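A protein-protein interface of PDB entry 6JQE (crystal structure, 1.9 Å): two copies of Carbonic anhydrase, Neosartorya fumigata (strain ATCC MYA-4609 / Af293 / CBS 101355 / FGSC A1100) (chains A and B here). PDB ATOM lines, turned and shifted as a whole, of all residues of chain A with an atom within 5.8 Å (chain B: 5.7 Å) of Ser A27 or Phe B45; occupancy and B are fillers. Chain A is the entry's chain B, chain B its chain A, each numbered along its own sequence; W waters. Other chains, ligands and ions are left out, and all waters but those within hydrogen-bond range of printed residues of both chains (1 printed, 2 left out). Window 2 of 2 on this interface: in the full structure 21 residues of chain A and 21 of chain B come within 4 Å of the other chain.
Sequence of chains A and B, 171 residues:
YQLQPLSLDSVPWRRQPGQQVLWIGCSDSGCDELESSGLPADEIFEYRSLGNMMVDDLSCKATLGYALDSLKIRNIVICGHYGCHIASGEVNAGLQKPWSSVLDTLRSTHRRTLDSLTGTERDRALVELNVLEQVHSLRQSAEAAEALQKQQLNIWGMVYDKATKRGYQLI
The backbone carbonyl oxygen (O) of Glu B46 sits at hydrogen-bond distance from the side-chain hydroxyl (OG) of Ser A27 (2.8 Å).
The side-chain carboxylate of Glu B46 lies within salt-bridge range of the guanidinium group of Arg A48, 3.7 Å away.
N of Trp B23 sits at hydrogen-bond distance from O of Phe B45, at 2.8 Å.
The backbone carbonyl oxygen of Val B21 lies within hydrogen-bond range of the backbone NH of Phe B45 (2.9 Å).
N of Ser A27 sits at hydrogen-bond distance from O of Ser A49, 3.0 Å away.
N of Leu B71 is in hydrogen-bond range of O of Tyr B66.
O of Cys A26 is in hydrogen-bond range of NH1 of Arg A48, 2.9 Å away.
The backbone carbonyl oxygen (O) of Trp B23 sits at hydrogen-bond distance from the backbone NH (N) of Tyr B47.
CB of Ser A27 touches CZ of Phe B45, at 3.5 Å.
CD1 of Tyr B47 touches O of Arg A48, at 3.3 Å.
CZ of Phe B45 touches CD2 of Leu A50, 3.7 Å away.
Leu A50 touches Thr B63.
Ile A86 touches Tyr B66 (CG1 to OH, 3.7 Å).
Of the printed residues of chain B, Ser A27 touches Phe B45 (3.5 Å) and Glu B46 (2.8 Å).
Printed residues of chain B within 4 Å of Arg A48: Glu B46 and Tyr B47.
Printed residues of chain B within 4 Å of Ile A86: Tyr B66 (3.7 Å).
Of the printed residues of chain A, Phe B45 touches Ser A27 and Leu A50.
Printed residues of chain A within 4 Å of Glu B46: Ser A27 and Arg A48.
Of the printed residues of chain A, Tyr B47 touches Arg A48.
Of the printed residues of chain A, Thr B63 touches Leu A50 (3.7 Å).
Ile B73 touches none of the printed residues of chain A.
The nearest printed residue of chain A that does not touch Phe B45 is Asp A28 (4.02 Å).
Of the 11 printed residues of chain A, 4 touch a printed residue of chain B.
Hydrophobic or aromatic side chains of chain A within 4 Å of the printed part of chain B: Leu A50 and Ile A86.
Of the 16 printed residues of chain B, 5 touch a printed residue of chain A.
Printed residues of chain B that touch a printed residue of chain A: Phe B45, Glu B46, Tyr B47, Thr B63 and Tyr B66.
Among the printed residues, Asp or Glu carboxylates within 4 Å of a Lys or Arg side-chain nitrogen of the other chain: Arg A48 with Glu B46 (3.7 Å).
No position is printed for both chains.
Of the 7 pairs that touch across the chains among the printed residues, none has its exchanged pair printed and touching as well.
Water W1 bridges OH of Tyr B66 and OD2 of Asp A28.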
ATOM      1  N   GLY A  25      -1.259 -29.212 -32.503  1.00  0.00           N
ATOM      2  CA  GLY A  25      -1.300 -28.386 -31.289  1.00  0.00           C
ATOM      3  C   GLY A  25      -2.508 -28.709 -30.438  1.00  0.00           C
ATOM      4  O   GLY A  25      -3.350 -29.496 -30.865  1.00  0.00           O
ATOM      5  N   CYS A  26      -2.617 -28.069 -29.275  1.00  0.00           N
ATOM      6  CA  CYS A  26      -3.709 -28.326 -28.319  1.00  0.00           C
ATOM      7  C   CYS A  26      -4.866 -27.317 -28.502  1.00  0.00           C
ATOM      8  O   CYS A  26      -4.629 -26.113 -28.684  1.00  0.00           O
ATOM      9  CB  CYS A  26      -3.194 -28.288 -26.888  1.00  0.00           C
ATOM     10  SG  CYS A  26      -4.490 -28.784 -25.732  1.00  0.00           S
ATOM     11  N   SER A  27      -6.080 -27.828 -28.363  1.00  0.00           N
ATOM     12  CA  SER A  27      -7.385 -27.109 -28.356  1.00  0.00           C
ATOM     13  C   SER A  27      -7.456 -25.965 -27.353  1.00  0.00           C
ATOM     14  O   SER A  27      -8.161 -24.987 -27.682  1.00  0.00           O
ATOM     15  CB  SER A  27      -8.483 -28.132 -28.113  1.00  0.00           C
ATOM     16  OG  SER A  27      -8.599 -28.914 -29.278  1.00  0.00           O
ATOM     17  N   ASP A  28      -6.799 -26.043 -26.184  1.00  0.00           N
ATOM     18  CA  ASP A  28      -6.839 -24.935 -25.185  1.00  0.00           C
ATOM     19  C   ASP A  28      -5.554 -24.082 -25.268  1.00  0.00           C
ATOM     20  O   ASP A  28      -5.316 -23.294 -24.342  1.00  0.00           O
ATOM     21  CB  ASP A  28      -7.148 -25.436 -23.767  1.00  0.00           C
ATOM     22  CG  ASP A  28      -6.075 -26.289 -23.095  1.00  0.00           C
ATOM     23  OD1 ASP A  28      -4.874 -26.178 -23.503  1.00  0.00           O
ATOM     24  OD2 ASP A  28      -6.382 -27.096 -22.175  1.00  0.00           O
ATOM     25  N   SER A  29      -4.747 -24.223 -26.324  1.00  0.00           N
ATOM     26  CA  SER A  29      -3.631 -23.289 -26.645  1.00  0.00           C
ATOM     27  C   SER A  29      -4.065 -22.314 -27.755  1.00  0.00           C
ATOM     28  O   SER A  29      -4.696 -22.766 -28.707  1.00  0.00           O
ATOM     29  CB  SER A  29      -2.390 -24.036 -27.046  1.00  0.00           C
ATOM     30  OG  SER A  29      -1.333 -23.151 -27.379  1.00  0.00           O
ATOM     31  N   ARG A  48      -5.597 -29.336 -34.567  1.00  0.00           N
ATOM     32  CA  ARG A  48      -5.678 -28.864 -33.158  1.00  0.00           C
ATOM     33  C   ARG A  48      -6.681 -29.746 -32.415  1.00  0.00           C
ATOM     34  O   ARG A  48      -7.865 -29.771 -32.800  1.00  0.00           O
ATOM     35  CB  ARG A  48      -5.965 -27.372 -33.098  1.00  0.00           C
ATOM     36  CG  ARG A  48      -5.656 -26.757 -31.742  1.00  0.00           C
ATOM     37  CD  ARG A  48      -5.590 -25.241 -31.826  1.00  0.00           C
ATOM     38  NE  ARG A  48      -4.405 -24.776 -32.537  1.00  0.00           N
ATOM     39  CZ  ARG A  48      -3.180 -24.669 -32.032  1.00  0.00           C
ATOM     40  NH1 ARG A  48      -2.916 -24.988 -30.770  1.00  0.00           N
ATOM     41  NH2 ARG A  48      -2.197 -24.230 -32.802  1.00  0.00           N
ATOM     42  N   SER A  49      -6.184 -30.459 -31.397  1.00  0.00           N
ATOM     43  CA  SER A  49      -6.899 -31.592 -30.763  1.00  0.00           C
ATOM     44  C   SER A  49      -6.688 -31.558 -29.256  1.00  0.00           C
ATOM     45  O   SER A  49      -5.859 -30.782 -28.776  1.00  0.00           O
ATOM     46  CB  SER A  49      -6.375 -32.883 -31.303  1.00  0.00           C
ATOM     47  OG  SER A  49      -4.940 -32.956 -31.045  1.00  0.00           O
ATOM     48  N   LEU A  50      -7.387 -32.442 -28.557  1.00  0.00           N
ATOM     49  CA  LEU A  50      -7.250 -32.633 -27.093  1.00  0.00           C
ATOM     50  C   LEU A  50      -5.802 -33.006 -26.735  1.00  0.00           C
ATOM     51  O   LEU A  50      -5.309 -34.068 -27.179  1.00  0.00           O
ATOM     52  CB  LEU A  50      -8.239 -33.725 -26.672  1.00  0.00           C
ATOM     53  CG  LEU A  50      -9.706 -33.443 -26.971  1.00  0.00           C
ATOM     54  CD1 LEU A  50     -10.568 -34.666 -26.653  1.00  0.00           C
ATOM     55  CD2 LEU A  50     -10.182 -32.230 -26.193  1.00  0.00           C
ATOM     56  N   GLY A  51      -5.144 -32.136 -25.970  1.00  0.00           N
ATOM     57  CA  GLY A  51      -3.794 -32.307 -25.418  1.00  0.00           C
ATOM     58  C   GLY A  51      -2.722 -32.505 -26.478  1.00  0.00           C
ATOM     59  O   GLY A  51      -1.749 -33.170 -26.145  1.00  0.00           O
ATOM     60  N   ASN A  52      -2.881 -31.925 -27.684  1.00  0.00           N
ATOM     61  CA  ASN A  52      -1.920 -32.042 -28.813  1.00  0.00           C
ATOM     62  C   ASN A  52      -1.556 -33.530 -28.974  1.00  0.00           C
ATOM     63  O   ASN A  52      -0.394 -33.842 -29.214  1.00  0.00           O
ATOM     64  CB  ASN A  52      -0.687 -31.127 -28.661  1.00  0.00           C
ATOM     65  CG  ASN A  52      -0.040 -31.104 -27.291  1.00  0.00           C
ATOM     66  OD1 ASN A  52      -0.430 -30.259 -26.494  1.00  0.00           O
ATOM     67  ND2 ASN A  52       1.010 -31.913 -27.074  1.00  0.00           N
ATOM     68  N   ILE A  86      -5.329 -29.998 -20.024  1.00  0.00           N
ATOM     69  CA  ILE A  86      -5.535 -31.426 -20.374  1.00  0.00           C
ATOM     70  C   ILE A  86      -4.287 -32.220 -19.958  1.00  0.00           C
ATOM     71  O   ILE A  86      -4.439 -33.242 -19.287  1.00  0.00           O
ATOM     72  CB  ILE A  86      -5.913 -31.560 -21.866  1.00  0.00           C
ATOM     73  CG1 ILE A  86      -7.282 -30.919 -22.140  1.00  0.00           C
ATOM     74  CG2 ILE A  86      -5.899 -33.011 -22.295  1.00  0.00           C
ATOM     75  CD1 ILE A  86      -7.547 -30.560 -23.575  1.00  0.00           C
ATOM     76  N   GLN B  20     -16.585 -20.033 -22.665  1.00  0.00           N
ATOM     77  CA  GLN B  20     -15.729 -20.603 -23.741  1.00  0.00           C
ATOM     78  C   GLN B  20     -16.596 -21.059 -24.909  1.00  0.00           C
ATOM     79  O   GLN B  20     -17.684 -21.613 -24.686  1.00  0.00           O
ATOM     80  CB  GLN B  20     -14.858 -21.750 -23.223  1.00  0.00           C
ATOM     81  CG  GLN B  20     -13.413 -21.329 -23.007  1.00  0.00           C
ATOM     82  CD  GLN B  20     -12.671 -22.384 -22.233  1.00  0.00           C
ATOM     83  OE1 GLN B  20     -13.014 -22.687 -21.094  1.00  0.00           O
ATOM     84  NE2 GLN B  20     -11.670 -22.965 -22.865  1.00  0.00           N
ATOM     85  N   VAL B  21     -16.122 -20.822 -26.121  1.00  0.00           N
ATOM     86  CA  VAL B  21     -16.812 -21.246 -27.374  1.00  0.00           C
ATOM     87  C   VAL B  21     -15.990 -22.355 -28.042  1.00  0.00           C
ATOM     88  O   VAL B  21     -14.744 -22.195 -28.151  1.00  0.00           O
ATOM     89  CB  VAL B  21     -16.989 -20.024 -28.277  1.00  0.00           C
ATOM     90  CG1 VAL B  21     -17.505 -20.407 -29.651  1.00  0.00           C
ATOM     91  CG2 VAL B  21     -17.882 -18.994 -27.598  1.00  0.00           C
ATOM     92  N   LEU B  22     -16.638 -23.451 -28.431  1.00  0.00           N
ATOM     93  CA  LEU B  22     -15.956 -24.494 -29.226  1.00  0.00           C
ATOM     94  C   LEU B  22     -15.967 -24.030 -30.683  1.00  0.00           C
ATOM     95  O   LEU B  22     -17.043 -23.862 -31.245  1.00  0.00           O
ATOM     96  CB  LEU B  22     -16.667 -25.831 -29.048  1.00  0.00           C
ATOM     97  CG  LEU B  22     -16.292 -26.947 -30.014  1.00  0.00           C
ATOM     98  CD1 LEU B  22     -14.800 -27.257 -29.968  1.00  0.00           C
ATOM     99  CD2 LEU B  22     -17.072 -28.192 -29.635  1.00  0.00           C
ATOM    100  N   TRP B  23     -14.797 -23.759 -31.209  1.00  0.00           N
ATOM    101  CA  TRP B  23     -14.575 -23.245 -32.576  1.00  0.00           C
ATOM    102  C   TRP B  23     -14.082 -24.409 -33.420  1.00  0.00           C
ATOM    103  O   TRP B  23     -13.008 -24.933 -33.077  1.00  0.00           O
ATOM    104  CB  TRP B  23     -13.578 -22.099 -32.544  1.00  0.00           C
ATOM    105  CG  TRP B  23     -13.492 -21.378 -33.852  1.00  0.00           C
ATOM    106  CD1 TRP B  23     -12.813 -21.750 -34.968  1.00  0.00           C
ATOM    107  CD2 TRP B  23     -14.233 -20.204 -34.208  1.00  0.00           C
ATOM    108  NE1 TRP B  23     -13.019 -20.843 -35.977  1.00  0.00           N
ATOM    109  CE2 TRP B  23     -13.902 -19.895 -35.547  1.00  0.00           C
ATOM    110  CE3 TRP B  23     -15.118 -19.382 -33.514  1.00  0.00           C
ATOM    111  CZ2 TRP B  23     -14.403 -18.770 -36.187  1.00  0.00           C
ATOM    112  CZ3 TRP B  23     -15.626 -18.275 -34.155  1.00  0.00           C
ATOM    113  CH2 TRP B  23     -15.284 -17.990 -35.474  1.00  0.00           C
ATOM    114  N   ILE B  24     -14.864 -24.823 -34.415  1.00  0.00           N
ATOM    115  CA  ILE B  24     -14.519 -25.922 -35.341  1.00  0.00           C
ATOM    116  C   ILE B  24     -14.108 -25.291 -36.673  1.00  0.00           C
ATOM    117  O   ILE B  24     -14.956 -24.688 -37.325  1.00  0.00           O
ATOM    118  CB  ILE B  24     -15.684 -26.909 -35.473  1.00  0.00           C
ATOM    119  CG1 ILE B  24     -16.073 -27.520 -34.111  1.00  0.00           C
ATOM    120  CG2 ILE B  24     -15.325 -27.934 -36.515  1.00  0.00           C
ATOM    121  CD1 ILE B  24     -17.365 -28.298 -34.124  1.00  0.00           C
ATOM    122  N   ALA B  41      -8.822 -14.496 -27.192  1.00  0.00           N
ATOM    123  CA  ALA B  41      -8.138 -15.805 -27.305  1.00  0.00           C
ATOM    124  C   ALA B  41      -8.547 -16.730 -26.145  1.00  0.00           C
ATOM    125  O   ALA B  41      -8.729 -17.930 -26.391  1.00  0.00           O
ATOM    126  CB  ALA B  41      -6.639 -15.599 -27.376  1.00  0.00           C
ATOM    127  N   GLU B  43     -11.313 -17.150 -24.665  1.00  0.00           N
ATOM    128  CA  GLU B  43     -12.715 -17.644 -24.772  1.00  0.00           C
ATOM    129  C   GLU B  43     -12.842 -18.639 -25.936  1.00  0.00           C
ATOM    130  O   GLU B  43     -13.983 -19.024 -26.282  1.00  0.00           O
ATOM    131  CB  GLU B  43     -13.663 -16.452 -24.945  1.00  0.00           C
ATOM    132  CG  GLU B  43     -13.767 -15.568 -23.705  1.00  0.00           C
ATOM    133  CD  GLU B  43     -14.734 -14.378 -23.811  1.00  0.00           C
ATOM    134  OE1 GLU B  43     -15.537 -14.298 -24.797  1.00  0.00           O
ATOM    135  OE2 GLU B  43     -14.700 -13.524 -22.890  1.00  0.00           O
ATOM    136  N   ILE B  44     -11.725 -19.072 -26.506  1.00  0.00           N
ATOM    137  CA  ILE B  44     -11.713 -19.968 -27.695  1.00  0.00           C
ATOM    138  C   ILE B  44     -11.143 -21.323 -27.279  1.00  0.00           C
ATOM    139  O   ILE B  44     -10.004 -21.369 -26.816  1.00  0.00           O
ATOM    140  CB  ILE B  44     -10.926 -19.360 -28.867  1.00  0.00           C
ATOM    141  CG1 ILE B  44     -11.513 -18.005 -29.283  1.00  0.00           C
ATOM    142  CG2 ILE B  44     -10.917 -20.340 -30.025  1.00  0.00           C
ATOM    143  CD1 ILE B  44     -10.673 -17.228 -30.265  1.00  0.00           C
ATOM    144  N   PHE B  45     -11.930 -22.374 -27.479  1.00  0.00           N
ATOM    145  CA  PHE B  45     -11.476 -23.787 -27.472  1.00  0.00           C
ATOM    146  C   PHE B  45     -11.541 -24.275 -28.919  1.00  0.00           C
ATOM    147  O   PHE B  45     -12.660 -24.357 -29.466  1.00  0.00           O
ATOM    148  CB  PHE B  45     -12.366 -24.593 -26.533  1.00  0.00           C
ATOM    149  CG  PHE B  45     -11.904 -25.997 -26.294  1.00  0.00           C
ATOM    150  CD1 PHE B  45     -10.809 -26.255 -25.486  1.00  0.00           C
ATOM    151  CD2 PHE B  45     -12.556 -27.066 -26.898  1.00  0.00           C
ATOM    152  CE1 PHE B  45     -10.398 -27.560 -25.250  1.00  0.00           C
ATOM    153  CE2 PHE B  45     -12.142 -28.365 -26.661  1.00  0.00           C
ATOM    154  CZ  PHE B  45     -11.065 -28.604 -25.832  1.00  0.00           C
ATOM    155  N   GLU B  46     -10.383 -24.503 -29.547  1.00  0.00           N
ATOM    156  CA  GLU B  46     -10.270 -24.602 -31.021  1.00  0.00           C
ATOM    157  C   GLU B  46     -10.063 -26.058 -31.405  1.00  0.00           C
ATOM    158  O   GLU B  46      -9.113 -26.658 -30.911  1.00  0.00           O
ATOM    159  CB  GLU B  46      -9.159 -23.657 -31.491  1.00  0.00           C
ATOM    160  CG  GLU B  46      -8.950 -23.619 -32.981  1.00  0.00           C
ATOM    161  CD  GLU B  46      -7.810 -22.703 -33.411  1.00  0.00           C
ATOM    162  OE1 GLU B  46      -7.054 -22.206 -32.543  1.00  0.00           O
ATOM    163  OE2 GLU B  46      -7.650 -22.510 -34.620  1.00  0.00           O
ATOM    164  N   TYR B  47     -10.986 -26.630 -32.190  1.00  0.00           N
ATOM    165  CA  TYR B  47     -10.830 -27.955 -32.834  1.00  0.00           C
ATOM    166  C   TYR B  47     -10.623 -27.695 -34.329  1.00  0.00           C
ATOM    167  O   TYR B  47     -11.542 -27.113 -34.965  1.00  0.00           O
ATOM    168  CB  TYR B  47     -12.030 -28.861 -32.532  1.00  0.00           C
ATOM    169  CG  TYR B  47     -11.875 -30.244 -33.111  1.00  0.00           C
ATOM    170  CD1 TYR B  47     -10.883 -31.092 -32.634  1.00  0.00           C
ATOM    171  CD2 TYR B  47     -12.667 -30.697 -34.158  1.00  0.00           C
ATOM    172  CE1 TYR B  47     -10.664 -32.340 -33.189  1.00  0.00           C
ATOM    173  CE2 TYR B  47     -12.476 -31.947 -34.722  1.00  0.00           C
ATOM    174  CZ  TYR B  47     -11.465 -32.771 -34.237  1.00  0.00           C
ATOM    175  OH  TYR B  47     -11.224 -34.006 -34.760  1.00  0.00           O
ATOM    176  N   THR B  63     -14.099 -34.655 -28.246  1.00  0.00           N
ATOM    177  CA  THR B  63     -13.903 -33.185 -28.201  1.00  0.00           C
ATOM    178  C   THR B  63     -15.231 -32.519 -27.832  1.00  0.00           C
ATOM    179  O   THR B  63     -15.261 -31.649 -26.914  1.00  0.00           O
ATOM    180  CB  THR B  63     -13.339 -32.639 -29.515  1.00  0.00           C
ATOM    181  OG1 THR B  63     -12.112 -33.331 -29.762  1.00  0.00           O
ATOM    182  CG2 THR B  63     -13.078 -31.157 -29.443  1.00  0.00           C
ATOM    183  N   TYR B  66     -15.868 -33.310 -24.085  1.00  0.00           N
ATOM    184  CA  TYR B  66     -15.013 -32.534 -23.159  1.00  0.00           C
ATOM    185  C   TYR B  66     -15.543 -31.109 -23.124  1.00  0.00           C
ATOM    186  O   TYR B  66     -15.647 -30.544 -22.046  1.00  0.00           O
ATOM    187  CB  TYR B  66     -13.536 -32.586 -23.574  1.00  0.00           C
ATOM    188  CG  TYR B  66     -12.633 -31.761 -22.701  1.00  0.00           C
ATOM    189  CD1 TYR B  66     -12.168 -32.234 -21.481  1.00  0.00           C
ATOM    190  CD2 TYR B  66     -12.234 -30.496 -23.080  1.00  0.00           C
ATOM    191  CE1 TYR B  66     -11.317 -31.490 -20.684  1.00  0.00           C
ATOM    192  CE2 TYR B  66     -11.384 -29.740 -22.294  1.00  0.00           C
ATOM    193  CZ  TYR B  66     -10.938 -30.220 -21.078  1.00  0.00           C
ATOM    194  OH  TYR B  66     -10.111 -29.453 -20.312  1.00  0.00           O
ATOM    195  N   ALA B  67     -15.868 -30.549 -24.285  1.00  0.00           N
ATOM    196  CA  ALA B  67     -16.418 -29.178 -24.388  1.00  0.00           C
ATOM    197  C   ALA B  67     -17.704 -29.052 -23.543  1.00  0.00           C
ATOM    198  O   ALA B  67     -17.816 -28.065 -22.796  1.00  0.00           O
ATOM    199  CB  ALA B  67     -16.657 -28.833 -25.836  1.00  0.00           C
ATOM    200  N   LEU B  71     -15.945 -28.185 -19.900  1.00  0.00           N
ATOM    201  CA  LEU B  71     -15.868 -26.708 -20.064  1.00  0.00           C
ATOM    202  C   LEU B  71     -17.265 -26.081 -19.958  1.00  0.00           C
ATOM    203  O   LEU B  71     -17.327 -24.837 -19.890  1.00  0.00           O
ATOM    204  CB  LEU B  71     -15.219 -26.396 -21.415  1.00  0.00           C
ATOM    205  CG  LEU B  71     -13.835 -26.996 -21.640  1.00  0.00           C
ATOM    206  CD1 LEU B  71     -13.237 -26.516 -22.955  1.00  0.00           C
ATOM    207  CD2 LEU B  71     -12.909 -26.674 -20.473  1.00  0.00           C
ATOM    208  N   ILE B  73     -19.522 -25.622 -22.270  1.00  0.00           N
ATOM    209  CA  ILE B  73     -19.656 -24.658 -23.399  1.00  0.00           C
ATOM    210  C   ILE B  73     -21.147 -24.559 -23.765  1.00  0.00           C
ATOM    211  O   ILE B  73     -21.859 -25.557 -23.618  1.00  0.00           O
ATOM    212  CB  ILE B  73     -18.710 -25.081 -24.541  1.00  0.00           C
ATOM    213  CG1 ILE B  73     -17.257 -24.880 -24.092  1.00  0.00           C
ATOM    214  CG2 ILE B  73     -18.997 -24.347 -25.842  1.00  0.00           C
ATOM    215  CD1 ILE B  73     -16.212 -25.132 -25.159  1.00  0.00           C
HETATM  216  O   HOH W   1      -9.052 -27.273 -21.518  1.00  0.00           O
